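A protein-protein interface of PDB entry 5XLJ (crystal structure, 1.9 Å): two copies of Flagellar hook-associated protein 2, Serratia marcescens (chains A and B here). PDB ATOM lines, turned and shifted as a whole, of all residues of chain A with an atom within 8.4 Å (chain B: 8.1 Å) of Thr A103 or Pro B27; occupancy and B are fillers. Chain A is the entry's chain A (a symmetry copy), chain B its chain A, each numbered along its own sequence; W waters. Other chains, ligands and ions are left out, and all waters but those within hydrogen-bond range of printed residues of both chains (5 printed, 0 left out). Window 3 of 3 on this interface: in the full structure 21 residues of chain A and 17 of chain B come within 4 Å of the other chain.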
ATOM      1  N   ALA A  40     -22.974  -4.443 -13.018  1.00  0.00           N
ATOM      2  CA  ALA A  40     -22.558  -5.429 -14.011  1.00  0.00           C
ATOM      3  C   ALA A  40     -21.255  -6.054 -13.556  1.00  0.00           C
ATOM      4  O   ALA A  40     -20.248  -5.330 -13.350  1.00  0.00           O
ATOM      5  CB  ALA A  40     -22.327  -4.758 -15.382  1.00  0.00           C
ATOM      6  N   GLN A  41     -21.222  -7.380 -13.451  1.00  0.00           N
ATOM      7  CA  GLN A  41     -19.995  -8.055 -13.082  1.00  0.00           C
ATOM      8  C   GLN A  41     -18.878  -7.732 -14.085  1.00  0.00           C
ATOM      9  O   GLN A  41     -19.145  -7.609 -15.283  1.00  0.00           O
ATOM     10  CB  GLN A  41     -20.207  -9.563 -13.057  1.00  0.00           C
ATOM     11  CG  GLN A  41     -18.983 -10.372 -12.596  1.00  0.00           C
ATOM     12  CD  GLN A  41     -19.227 -11.860 -12.710  1.00  0.00           C
ATOM     13  OE1 GLN A  41     -19.809 -12.298 -13.687  1.00  0.00           O
ATOM     14  NE2 GLN A  41     -18.755 -12.646 -11.728  1.00  0.00           N
ATOM     15  N   THR A  42     -17.667  -7.521 -13.574  1.00  0.00           N
ATOM     16  CA  THR A  42     -16.480  -7.334 -14.417  1.00  0.00           C
ATOM     17  C   THR A  42     -15.408  -8.322 -14.033  1.00  0.00           C
ATOM     18  O   THR A  42     -15.132  -8.518 -12.858  1.00  0.00           O
ATOM     19  CB  THR A  42     -15.904  -5.905 -14.341  1.00  0.00           C
ATOM     20  OG1 THR A  42     -16.892  -4.978 -14.797  1.00  0.00           O
ATOM     21  CG2 THR A  42     -14.688  -5.800 -15.261  1.00  0.00           C
ATOM     22  N   LEU A  43     -14.821  -8.953 -15.052  1.00  0.00           N
ATOM     23  CA  LEU A  43     -13.695  -9.868 -14.913  1.00  0.00           C
ATOM     24  C   LEU A  43     -12.528  -9.228 -15.615  1.00  0.00           C
ATOM     25  O   LEU A  43     -12.686  -8.758 -16.750  1.00  0.00           O
ATOM     26  CB  LEU A  43     -13.977 -11.191 -15.602  1.00  0.00           C
ATOM     27  CG  LEU A  43     -15.268 -11.898 -15.206  1.00  0.00           C
ATOM     28  CD1 LEU A  43     -15.412 -13.195 -16.046  1.00  0.00           C
ATOM     29  CD2 LEU A  43     -15.361 -12.191 -13.723  1.00  0.00           C
ATOM     30  N   ILE A  68     -18.208 -17.942 -24.033  1.00  0.00           N
ATOM     31  CA  ILE A  68     -18.625 -16.945 -23.066  1.00  0.00           C
ATOM     32  C   ILE A  68     -20.046 -17.285 -22.665  1.00  0.00           C
ATOM     33  O   ILE A  68     -20.895 -17.465 -23.542  1.00  0.00           O
ATOM     34  CB  ILE A  68     -18.662 -15.538 -23.692  1.00  0.00           C
ATOM     35  CG1 ILE A  68     -17.277 -15.167 -24.229  1.00  0.00           C
ATOM     36  CG2 ILE A  68     -19.201 -14.499 -22.637  1.00  0.00           C
ATOM     37  CD1 ILE A  68     -17.300 -13.886 -25.052  1.00  0.00           C
ATOM     38  N   ALA A  70     -23.126 -15.742 -20.381  1.00  0.00           N
ATOM     39  CA  ALA A  70     -23.534 -14.447 -19.828  1.00  0.00           C
ATOM     40  C   ALA A  70     -25.033 -14.260 -20.021  1.00  0.00           C
ATOM     41  O   ALA A  70     -25.692 -15.012 -20.768  1.00  0.00           O
ATOM     42  CB  ALA A  70     -22.694 -13.258 -20.509  1.00  0.00           C
ATOM     43  N   LEU A  91      -8.402  -9.884 -28.911  1.00  0.00           N
ATOM     44  CA  LEU A  91      -9.374 -10.586 -28.045  1.00  0.00           C
ATOM     45  C   LEU A  91     -10.527  -9.637 -27.728  1.00  0.00           C
ATOM     46  O   LEU A  91     -11.701 -10.014 -27.788  1.00  0.00           O
ATOM     47  CB  LEU A  91      -8.730 -11.058 -26.743  1.00  0.00           C
ATOM     48  CG  LEU A  91      -7.776 -12.249 -26.868  1.00  0.00           C
ATOM     49  CD1 LEU A  91      -6.867 -12.371 -25.650  1.00  0.00           C
ATOM     50  CD2 LEU A  91      -8.605 -13.535 -27.082  1.00  0.00           C
ATOM     51  N   ARG A  92     -10.180  -8.394 -27.405  1.00  0.00           N
ATOM     52  CA  ARG A  92     -11.175  -7.357 -27.178  1.00  0.00           C
ATOM     53  C   ARG A  92     -12.104  -7.191 -28.386  1.00  0.00           C
ATOM     54  O   ARG A  92     -13.330  -7.197 -28.227  1.00  0.00           O
ATOM     55  CB  ARG A  92     -10.501  -6.020 -26.880  1.00  0.00           C
ATOM     56  CG  ARG A  92     -11.496  -4.874 -26.791  1.00  0.00           C
ATOM     57  CD  ARG A  92     -10.851  -3.531 -26.959  1.00  0.00           C
ATOM     58  NE  ARG A  92     -10.381  -3.340 -28.327  1.00  0.00           N
ATOM     59  CZ  ARG A  92      -9.441  -2.469 -28.688  1.00  0.00           C
ATOM     60  NH1 ARG A  92      -8.875  -1.674 -27.801  1.00  0.00           N
ATOM     61  NH2 ARG A  92      -9.054  -2.399 -29.955  1.00  0.00           N
ATOM     62  N   ILE A  95     -14.317 -10.341 -28.849  1.00  0.00           N
ATOM     63  CA  ILE A  95     -15.349 -10.404 -27.835  1.00  0.00           C
ATOM     64  C   ILE A  95     -16.467  -9.398 -28.124  1.00  0.00           C
ATOM     65  O   ILE A  95     -17.648  -9.760 -28.091  1.00  0.00           O
ATOM     66  CB  ILE A  95     -14.762 -10.209 -26.430  1.00  0.00           C
ATOM     67  CG1 ILE A  95     -13.916 -11.442 -26.084  1.00  0.00           C
ATOM     68  CG2 ILE A  95     -15.902 -10.007 -25.386  1.00  0.00           C
ATOM     69  CD1 ILE A  95     -12.981 -11.257 -24.826  1.00  0.00           C
ATOM     70  N   ASN A  96     -16.111  -8.153 -28.439  1.00  0.00           N
ATOM     71  CA  ASN A  96     -17.124  -7.135 -28.711  1.00  0.00           C
ATOM     72  C   ASN A  96     -17.924  -7.491 -29.965  1.00  0.00           C
ATOM     73  O   ASN A  96     -19.167  -7.356 -29.992  1.00  0.00           O
ATOM     74  CB  ASN A  96     -16.513  -5.727 -28.819  1.00  0.00           C
ATOM     75  CG  ASN A  96     -16.100  -5.157 -27.441  1.00  0.00           C
ATOM     76  OD1 ASN A  96     -16.764  -5.409 -26.445  1.00  0.00           O
ATOM     77  ND2 ASN A  96     -14.988  -4.411 -27.391  1.00  0.00           N
ATOM     78  N   GLY A  97     -17.232  -7.982 -30.983  1.00  0.00           N
ATOM     79  CA  GLY A  97     -17.911  -8.391 -32.224  1.00  0.00           C
ATOM     80  C   GLY A  97     -18.842  -9.585 -32.082  1.00  0.00           C
ATOM     81  O   GLY A  97     -19.745  -9.769 -32.907  1.00  0.00           O
ATOM     82  N   LYS A  99     -21.041 -10.127 -29.682  1.00  0.00           N
ATOM     83  CA  LYS A  99     -22.330  -9.784 -29.047  1.00  0.00           C
ATOM     84  C   LYS A  99     -22.801 -10.926 -28.165  1.00  0.00           C
ATOM     85  O   LYS A  99     -23.843 -11.539 -28.402  1.00  0.00           O
ATOM     86  CB  LYS A  99     -23.395  -9.383 -30.084  1.00  0.00           C
ATOM     87  CG  LYS A  99     -23.057  -8.069 -30.839  1.00  0.00           C
ATOM     88  CD  LYS A  99     -24.136  -7.740 -31.866  1.00  0.00           C
ATOM     89  CE  LYS A  99     -23.777  -6.502 -32.709  1.00  0.00           C
ATOM     90  NZ  LYS A  99     -24.931  -6.147 -33.599  1.00  0.00           N
ATOM     91  N   ALA A 100     -21.992 -11.209 -27.149  1.00  0.00           N
ATOM     92  CA  ALA A 100     -22.113 -12.413 -26.329  1.00  0.00           C
ATOM     93  C   ALA A 100     -22.632 -12.077 -24.934  1.00  0.00           C
ATOM     94  O   ALA A 100     -22.557 -12.913 -24.027  1.00  0.00           O
ATOM     95  CB  ALA A 100     -20.717 -13.133 -26.255  1.00  0.00           C
ATOM     96  N   GLY A 101     -23.229 -10.895 -24.773  1.00  0.00           N
ATOM     97  CA  GLY A 101     -23.739 -10.457 -23.471  1.00  0.00           C
ATOM     98  C   GLY A 101     -22.677  -9.843 -22.554  1.00  0.00           C
ATOM     99  O   GLY A 101     -22.909  -9.661 -21.348  1.00  0.00           O
ATOM    100  N   VAL A 102     -21.514  -9.522 -23.122  1.00  0.00           N
ATOM    101  CA  VAL A 102     -20.441  -8.828 -22.409  1.00  0.00           C
ATOM    102  C   VAL A 102     -19.853  -7.770 -23.355  1.00  0.00           C
ATOM    103  O   VAL A 102     -20.091  -7.814 -24.602  1.00  0.00           O
ATOM    104  CB  VAL A 102     -19.292  -9.759 -21.897  1.00  0.00           C
ATOM    105  CG1 VAL A 102     -19.804 -10.858 -20.969  1.00  0.00           C
ATOM    106  CG2 VAL A 102     -18.496 -10.362 -23.086  1.00  0.00           C
ATOM    107  N   THR A 103     -19.126  -6.821 -22.759  1.00  0.00           N
ATOM    108  CA  THR A 103     -18.319  -5.855 -23.479  1.00  0.00           C
ATOM    109  C   THR A 103     -16.895  -5.935 -22.953  1.00  0.00           C
ATOM    110  O   THR A 103     -16.672  -6.316 -21.802  1.00  0.00           O
ATOM    111  CB  THR A 103     -18.857  -4.400 -23.303  1.00  0.00           C
ATOM    112  OG1 THR A 103     -18.748  -3.998 -21.918  1.00  0.00           O
ATOM    113  CG2 THR A 103     -20.323  -4.317 -23.775  1.00  0.00           C
ATOM    114  N   ALA A 104     -15.926  -5.584 -23.792  1.00  0.00           N
ATOM    115  CA  ALA A 104     -14.511  -5.723 -23.448  1.00  0.00           C
ATOM    116  C   ALA A 104     -13.802  -4.411 -23.705  1.00  0.00           C
ATOM    117  O   ALA A 104     -14.067  -3.746 -24.710  1.00  0.00           O
ATOM    118  CB  ALA A 104     -13.871  -6.856 -24.248  1.00  0.00           C
ATOM    119  N   SER A 105     -12.942  -4.022 -22.772  1.00  0.00           N
ATOM    120  CA  SER A 105     -12.119  -2.830 -22.920  1.00  0.00           C
ATOM    121  C   SER A 105     -10.748  -3.107 -22.315  1.00  0.00           C
ATOM    122  O   SER A 105     -10.608  -3.983 -21.465  1.00  0.00           O
ATOM    123  CB  SER A 105     -12.772  -1.624 -22.247  1.00  0.00           C
ATOM    124  OG  SER A 105     -12.893  -1.846 -20.846  1.00  0.00           O
ATOM    125  N   ILE A 106      -9.742  -2.353 -22.747  1.00  0.00           N
ATOM    126  CA  ILE A 106      -8.383  -2.532 -22.252  1.00  0.00           C
ATOM    127  C   ILE A 106      -8.055  -1.393 -21.287  1.00  0.00           C
ATOM    128  O   ILE A 106      -8.305  -0.226 -21.582  1.00  0.00           O
ATOM    129  CB  ILE A 106      -7.387  -2.586 -23.414  1.00  0.00           C
ATOM    130  CG1 ILE A 106      -7.594  -3.908 -24.143  1.00  0.00           C
ATOM    131  CG2 ILE A 106      -5.910  -2.406 -22.903  1.00  0.00           C
ATOM    132  CD1 ILE A 106      -6.850  -4.071 -25.359  1.00  0.00           C
ATOM    133  N   LEU A 116      -7.179  -6.691 -19.710  1.00  0.00           N
ATOM    134  CA  LEU A 116      -8.408  -6.746 -20.463  1.00  0.00           C
ATOM    135  C   LEU A 116      -9.559  -6.936 -19.479  1.00  0.00           C
ATOM    136  O   LEU A 116      -9.545  -7.878 -18.667  1.00  0.00           O
ATOM    137  CB  LEU A 116      -8.387  -7.893 -21.473  1.00  0.00           C
ATOM    138  CG  LEU A 116      -9.643  -8.127 -22.310  1.00  0.00           C
ATOM    139  CD1 LEU A 116      -9.908  -6.973 -23.292  1.00  0.00           C
ATOM    140  CD2 LEU A 116      -9.477  -9.468 -23.077  1.00  0.00           C
ATOM    141  N   ALA A 117     -10.542  -6.042 -19.541  1.00  0.00           N
ATOM    142  CA  ALA A 117     -11.698  -6.096 -18.629  1.00  0.00           C
ATOM    143  C   ALA A 117     -12.915  -6.522 -19.426  1.00  0.00           C
ATOM    144  O   ALA A 117     -13.211  -5.895 -20.427  1.00  0.00           O
ATOM    145  CB  ALA A 117     -11.944  -4.702 -18.006  1.00  0.00           C
ATOM    146  N   VAL A 118     -13.609  -7.563 -18.972  1.00  0.00           N
ATOM    147  CA  VAL A 118     -14.804  -8.079 -19.618  1.00  0.00           C
ATOM    148  C   VAL A 118     -15.964  -7.837 -18.651  1.00  0.00           C
ATOM    149  O   VAL A 118     -15.947  -8.348 -17.537  1.00  0.00           O
ATOM    150  CB  VAL A 118     -14.623  -9.568 -19.939  1.00  0.00           C
ATOM    151  CG1 VAL A 118     -15.923 -10.187 -20.606  1.00  0.00           C
ATOM    152  CG2 VAL A 118     -13.405  -9.773 -20.866  1.00  0.00           C
ATOM    153  N   SER A 119     -16.934  -7.022 -19.066  1.00  0.00           N
ATOM    154  CA  SER A 119     -18.037  -6.573 -18.203  1.00  0.00           C
ATOM    155  C   SER A 119     -19.345  -7.079 -18.777  1.00  0.00           C
ATOM    156  O   SER A 119     -19.531  -7.040 -19.994  1.00  0.00           O
ATOM    157  CB  SER A 119     -18.091  -5.035 -18.151  1.00  0.00           C
ATOM    158  OG  SER A 119     -16.878  -4.519 -17.581  1.00  0.00           O
ATOM    159  N   SER A 120     -20.256  -7.521 -17.918  1.00  0.00           N
ATOM    160  CA  SER A 120     -21.569  -7.910 -18.372  1.00  0.00           C
ATOM    161  C   SER A 120     -22.255  -6.729 -19.062  1.00  0.00           C
ATOM    162  O   SER A 120     -22.167  -5.604 -18.584  1.00  0.00           O
ATOM    163  CB  SER A 120     -22.443  -8.402 -17.210  1.00  0.00           C
ATOM    164  OG  SER A 120     -23.725  -8.786 -17.686  1.00  0.00           O
ATOM    165  N   SER A 121     -22.970  -7.012 -20.165  1.00  0.00           N
ATOM    166  CA  SER A 121     -23.789  -6.028 -20.853  1.00  0.00           C
ATOM    167  C   SER A 121     -25.040  -5.691 -20.050  1.00  0.00           C
ATOM    168  O   SER A 121     -25.701  -4.693 -20.281  1.00  0.00           O
ATOM    169  CB  SER A 121     -24.217  -6.575 -22.247  1.00  0.00           C
ATOM    170  OG  SER A 121     -23.048  -6.701 -23.022  1.00  0.00           O
ATOM    171  N   THR A 122     -25.380  -6.564 -19.128  1.00  0.00           N
ATOM    172  CA  THR A 122     -26.555  -6.413 -18.289  1.00  0.00           C
ATOM    173  C   THR A 122     -26.111  -6.381 -16.837  1.00  0.00           C
ATOM    174  O   THR A 122     -25.173  -7.081 -16.446  1.00  0.00           O
ATOM    175  CB  THR A 122     -27.502  -7.575 -18.529  1.00  0.00           C
ATOM    176  OG1 THR A 122     -26.807  -8.831 -18.359  1.00  0.00           O
ATOM    177  CG2 THR A 122     -28.094  -7.483 -19.964  1.00  0.00           C
ATOM    178  N   ILE A 129     -20.827 -14.125 -15.402  1.00  0.00           N
ATOM    179  CA  ILE A 129     -20.065 -14.472 -16.617  1.00  0.00           C
ATOM    180  C   ILE A 129     -19.183 -15.678 -16.325  1.00  0.00           C
ATOM    181  O   ILE A 129     -18.540 -15.754 -15.249  1.00  0.00           O
ATOM    182  CB  ILE A 129     -19.138 -13.318 -17.021  1.00  0.00           C
ATOM    183  CG1 ILE A 129     -19.903 -12.008 -17.222  1.00  0.00           C
ATOM    184  CG2 ILE A 129     -18.303 -13.672 -18.296  1.00  0.00           C
ATOM    185  CD1 ILE A 129     -19.016 -10.758 -17.178  1.00  0.00           C
ATOM    186  N   ASN B  22     -14.176   9.658 -27.361  1.00  0.00           N
ATOM    187  CA  ASN B  22     -14.112   9.680 -28.824  1.00  0.00           C
ATOM    188  C   ASN B  22     -14.543   8.313 -29.348  1.00  0.00           C
ATOM    189  O   ASN B  22     -14.985   7.450 -28.570  1.00  0.00           O
ATOM    190  CB  ASN B  22     -12.707  10.075 -29.312  1.00  0.00           C
ATOM    191  CG  ASN B  22     -11.645   9.083 -28.910  1.00  0.00           C
ATOM    192  OD1 ASN B  22     -11.844   7.869 -28.996  1.00  0.00           O
ATOM    193  ND2 ASN B  22     -10.506   9.590 -28.444  1.00  0.00           N
ATOM    194  N   ALA B  23     -14.417   8.126 -30.660  1.00  0.00           N
ATOM    195  CA  ALA B  23     -14.871   6.927 -31.347  1.00  0.00           C
ATOM    196  C   ALA B  23     -14.306   5.607 -30.799  1.00  0.00           C
ATOM    197  O   ALA B  23     -14.932   4.570 -30.985  1.00  0.00           O
ATOM    198  CB  ALA B  23     -14.562   7.056 -32.864  1.00  0.00           C
ATOM    199  N   LYS B  24     -13.149   5.648 -30.122  1.00  0.00           N
ATOM    200  CA  LYS B  24     -12.497   4.433 -29.585  1.00  0.00           C
ATOM    201  C   LYS B  24     -13.093   3.900 -28.282  1.00  0.00           C
ATOM    202  O   LYS B  24     -12.780   2.773 -27.868  1.00  0.00           O
ATOM    203  CB  LYS B  24     -11.000   4.683 -29.375  1.00  0.00           C
ATOM    204  N   ALA B  25     -13.917   4.700 -27.609  1.00  0.00           N
ATOM    205  CA  ALA B  25     -14.528   4.268 -26.354  1.00  0.00           C
ATOM    206  C   ALA B  25     -15.491   3.101 -26.616  1.00  0.00           C
ATOM    207  O   ALA B  25     -16.204   3.089 -27.623  1.00  0.00           O
ATOM    208  CB  ALA B  25     -15.260   5.436 -25.663  1.00  0.00           C
ATOM    209  N   VAL B  26     -15.505   2.135 -25.697  1.00  0.00           N
ATOM    210  CA  VAL B  26     -16.357   0.958 -25.807  1.00  0.00           C
ATOM    211  C   VAL B  26     -17.640   1.179 -25.026  1.00  0.00           C
ATOM    212  O   VAL B  26     -17.596   1.415 -23.806  1.00  0.00           O
ATOM    213  CB  VAL B  26     -15.652  -0.321 -25.270  1.00  0.00           C
ATOM    214  CG1 VAL B  26     -16.599  -1.521 -25.355  1.00  0.00           C
ATOM    215  CG2 VAL B  26     -14.373  -0.604 -26.049  1.00  0.00           C
ATOM    216  N   PRO B  27     -18.787   1.122 -25.709  1.00  0.00           N
ATOM    217  CA  PRO B  27     -20.044   1.226 -24.976  1.00  0.00           C
ATOM    218  C   PRO B  27     -20.176   0.128 -23.934  1.00  0.00           C
ATOM    219  O   PRO B  27     -19.904  -1.035 -24.229  1.00  0.00           O
ATOM    220  CB  PRO B  27     -21.101   1.053 -26.074  1.00  0.00           C
ATOM    221  CG  PRO B  27     -20.410   1.505 -27.330  1.00  0.00           C
ATOM    222  CD  PRO B  27     -19.013   1.013 -27.164  1.00  0.00           C
ATOM    223  N   GLY B  28     -20.570   0.488 -22.724  1.00  0.00           N
ATOM    224  CA  GLY B  28     -20.696  -0.513 -21.682  1.00  0.00           C
ATOM    225  C   GLY B  28     -20.932   0.050 -20.305  1.00  0.00           C
ATOM    226  O   GLY B  28     -21.113   1.254 -20.140  1.00  0.00           O
ATOM    227  N   ASN B  29     -20.923  -0.853 -19.326  1.00  0.00           N
ATOM    228  CA  ASN B  29     -21.196  -0.504 -17.937  1.00  0.00           C
ATOM    229  C   ASN B  29     -19.885  -0.323 -17.187  1.00  0.00           C
ATOM    230  O   ASN B  29     -19.049  -1.212 -17.215  1.00  0.00           O
ATOM    231  CB  ASN B  29     -22.035  -1.612 -17.305  1.00  0.00           C
ATOM    232  CG  ASN B  29     -23.409  -1.743 -17.963  1.00  0.00           C
ATOM    233  OD1 ASN B  29     -24.131  -0.753 -18.111  1.00  0.00           O
ATOM    234  ND2 ASN B  29     -23.749  -2.943 -18.385  1.00  0.00           N
ATOM    235  N   TYR B  30     -19.723   0.819 -16.520  1.00  0.00           N
ATOM    236  CA  TYR B  30     -18.540   1.119 -15.709  1.00  0.00           C
ATOM    237  C   TYR B  30     -18.911   1.594 -14.306  1.00  0.00           C
ATOM    238  O   TYR B  30     -19.939   2.238 -14.130  1.00  0.00           O
ATOM    239  CB  TYR B  30     -17.659   2.175 -16.400  1.00  0.00           C
ATOM    240  CG  TYR B  30     -17.241   1.742 -17.782  1.00  0.00           C
ATOM    241  CD1 TYR B  30     -18.094   1.921 -18.861  1.00  0.00           C
ATOM    242  CD2 TYR B  30     -16.008   1.126 -18.008  1.00  0.00           C
ATOM    243  CE1 TYR B  30     -17.754   1.498 -20.138  1.00  0.00           C
ATOM    244  CE2 TYR B  30     -15.640   0.714 -19.299  1.00  0.00           C
ATOM    245  CZ  TYR B  30     -16.532   0.898 -20.360  1.00  0.00           C
ATOM    246  OH  TYR B  30     -16.220   0.478 -21.651  1.00  0.00           O
ATOM    247  N   ASN B 169     -13.768   0.037 -13.002  1.00  0.00           N
ATOM    248  CA  ASN B 169     -14.279  -1.324 -12.917  1.00  0.00           C
ATOM    249  C   ASN B 169     -13.360  -2.214 -12.084  1.00  0.00           C
ATOM    250  O   ASN B 169     -12.987  -3.316 -12.480  1.00  0.00           O
ATOM    251  CB  ASN B 169     -14.532  -1.903 -14.308  1.00  0.00           C
ATOM    252  CG  ASN B 169     -15.957  -1.635 -14.818  1.00  0.00           C
ATOM    253  OD1 ASN B 169     -16.880  -1.344 -14.047  1.00  0.00           O
ATOM    254  ND2 ASN B 169     -16.146  -1.782 -16.120  1.00  0.00           N
ATOM    255  N   VAL B 187     -11.361   7.377 -23.736  1.00  0.00           N
ATOM    256  CA  VAL B 187     -11.959   8.038 -22.578  1.00  0.00           C
ATOM    257  C   VAL B 187     -10.953   8.898 -21.817  1.00  0.00           C
ATOM    258  O   VAL B 187      -9.827   8.471 -21.540  1.00  0.00           O
ATOM    259  CB  VAL B 187     -12.582   7.003 -21.615  1.00  0.00           C
ATOM    260  CG1 VAL B 187     -13.166   7.686 -20.379  1.00  0.00           C
ATOM    261  CG2 VAL B 187     -13.647   6.155 -22.350  1.00  0.00           C
ATOM    262  N   LEU B 203     -21.238   4.778 -14.523  1.00  0.00           N
ATOM    263  CA  LEU B 203     -21.014   5.418 -15.802  1.00  0.00           C
ATOM    264  C   LEU B 203     -21.473   4.443 -16.884  1.00  0.00           C
ATOM    265  O   LEU B 203     -21.075   3.282 -16.874  1.00  0.00           O
ATOM    266  CB  LEU B 203     -19.532   5.758 -15.968  1.00  0.00           C
ATOM    267  CG  LEU B 203     -19.060   6.216 -17.357  1.00  0.00           C
ATOM    268  CD1 LEU B 203     -19.642   7.570 -17.713  1.00  0.00           C
ATOM    269  CD2 LEU B 203     -17.545   6.253 -17.421  1.00  0.00           C
ATOM    270  N   VAL B 204     -22.340   4.901 -17.784  1.00  0.00           N
ATOM    271  CA  VAL B 204     -22.675   4.116 -18.975  1.00  0.00           C
ATOM    272  C   VAL B 204     -22.147   4.866 -20.193  1.00  0.00           C
ATOM    273  O   VAL B 204     -22.456   6.046 -20.382  1.00  0.00           O
ATOM    274  CB  VAL B 204     -24.193   3.874 -19.115  1.00  0.00           C
ATOM    275  CG1 VAL B 204     -24.493   3.011 -20.365  1.00  0.00           C
ATOM    276  CG2 VAL B 204     -24.745   3.200 -17.859  1.00  0.00           C
ATOM    277  N   ILE B 205     -21.323   4.207 -21.003  1.00  0.00           N
ATOM    278  CA  ILE B 205     -20.921   4.784 -22.291  1.00  0.00           C
ATOM    279  C   ILE B 205     -21.827   4.161 -23.343  1.00  0.00           C
ATOM    280  O   ILE B 205     -22.093   2.968 -23.282  1.00  0.00           O
ATOM    281  CB  ILE B 205     -19.440   4.505 -22.608  1.00  0.00           C
ATOM    282  CG1 ILE B 205     -18.552   5.086 -21.504  1.00  0.00           C
ATOM    283  CG2 ILE B 205     -19.079   5.066 -23.972  1.00  0.00           C
ATOM    284  CD1 ILE B 205     -17.101   4.732 -21.630  1.00  0.00           C
ATOM    285  N   SER B 206     -22.341   4.963 -24.283  1.00  0.00           N
ATOM    286  CA  SER B 206     -23.243   4.422 -25.311  1.00  0.00           C
ATOM    287  C   SER B 206     -22.996   5.005 -26.693  1.00  0.00           C
ATOM    288  O   SER B 206     -21.859   5.316 -27.033  1.00  0.00           O
ATOM    289  CB  SER B 206     -24.691   4.645 -24.906  1.00  0.00           C
ATOM    290  OG  SER B 206     -24.962   6.021 -24.770  1.00  0.00           O
HETATM  291  O   HOH W   1     -20.727  -3.492 -20.294  1.00  0.00           O
HETATM  292  O   HOH W   2     -16.399  -2.442 -21.710  1.00  0.00           O
HETATM  293  O   HOH W   3     -19.392  -2.699 -13.896  1.00  0.00           O
HETATM  294  O   HOH W   4     -14.091  -1.745 -17.782  1.00  0.00           O
HETATM  295  O   HOH W   5     -11.303   0.441 -27.357  1.00  0.00           O
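O of Ser A120 sits at hydrogen-bond distance from ND2 of Asn B29 (3.1 Å).
The side-chain amide nitrogen (ND2) of Asn B29 sits at hydrogen-bond distance from the backbone carbonyl oxygen (O) of Ser A121.
OG of Ser A119 lies within hydrogen-bond range of ND2 of Asn B169, at 3.2 Å.
OD1 of Asn A96 sits at hydrogen-bond distance from N of Ala A104 (2.8 Å).
The backbone carbonyl oxygen (O) of Ile B205 lies within hydrogen-bond range of the backbone NH (N) of Gly B28 (3.0 Å).
The backbone NH of Val A102 sits at hydrogen-bond distance from the side-chain hydroxyl of Ser A121 (3.2 Å).
O of Gln A41 sits at hydrogen-bond distance from N of Ser A120 (2.9 Å).
ND2 of Asn A96 sits at hydrogen-bond distance from O of Arg A92, 3.3 Å away.
OG of Ser A120 sits at hydrogen-bond distance from O of Thr A122 (2.6 Å).
Among the printed residues, merely in contact across the chains: Thr A103 with Pro B27 (3.3 Å), Ala A104 with Val B26 (3.4 Å), Thr A42 with Asn B169 (3.5 Å), Ala A40 with Asn B29 (3.7 Å), Asn A96 with Val B26 (3.9 Å), Ser A119 with Asn B29 (3.97 Å) and Thr A103 with Gly B28 (3.999 Å).
Pro B27 touches one residue of chain A.
Of the printed residues of chain A, Gly B28 touches Thr A103 (3.999 Å).
Of the printed residues of chain A, Asn B169 touches Thr A42 (3.5 Å) and Ser A119 (3.2 Å).
Of the 27 printed residues of chain A, 8 touch a printed residue of chain B.
Hydrophobic or aromatic side chains of chain A within 4 Å of the printed part of chain B: Ala A40.
Among the printed residues, 10 pairs touch across the chains.
Among the printed residues, no Asp or Glu carboxylate lies within 4 Å of a Lys or Arg side-chain nitrogen of the other chain.
No position is printed for both chains.
Water W1 lies within hydrogen-bond range of OG1 of Thr A103 (2.6 Å), N of Asn B29 (2.8 Å) and O of Ser A120 (3.1 Å).
Water W4 bridges the side-chain amide nitrogen of Asn B169 (2.6 Å) and the side-chain hydroxyl of Ser A105 (3.3 Å).
Water W5 lies within hydrogen-bond range of O of Lys B24 (2.8 Å) and NH1 of Arg A92 (3.3 Å).
Water W3 bridges O of Ala A40 (2.8 Å) and OD1 of Asn B169 (2.9 Å).
Water W2 lies within hydrogen-bond range of the side-chain hydroxyl (OG1) of Thr A103 and the side-chain hydroxyl (OH) of Tyr B30.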
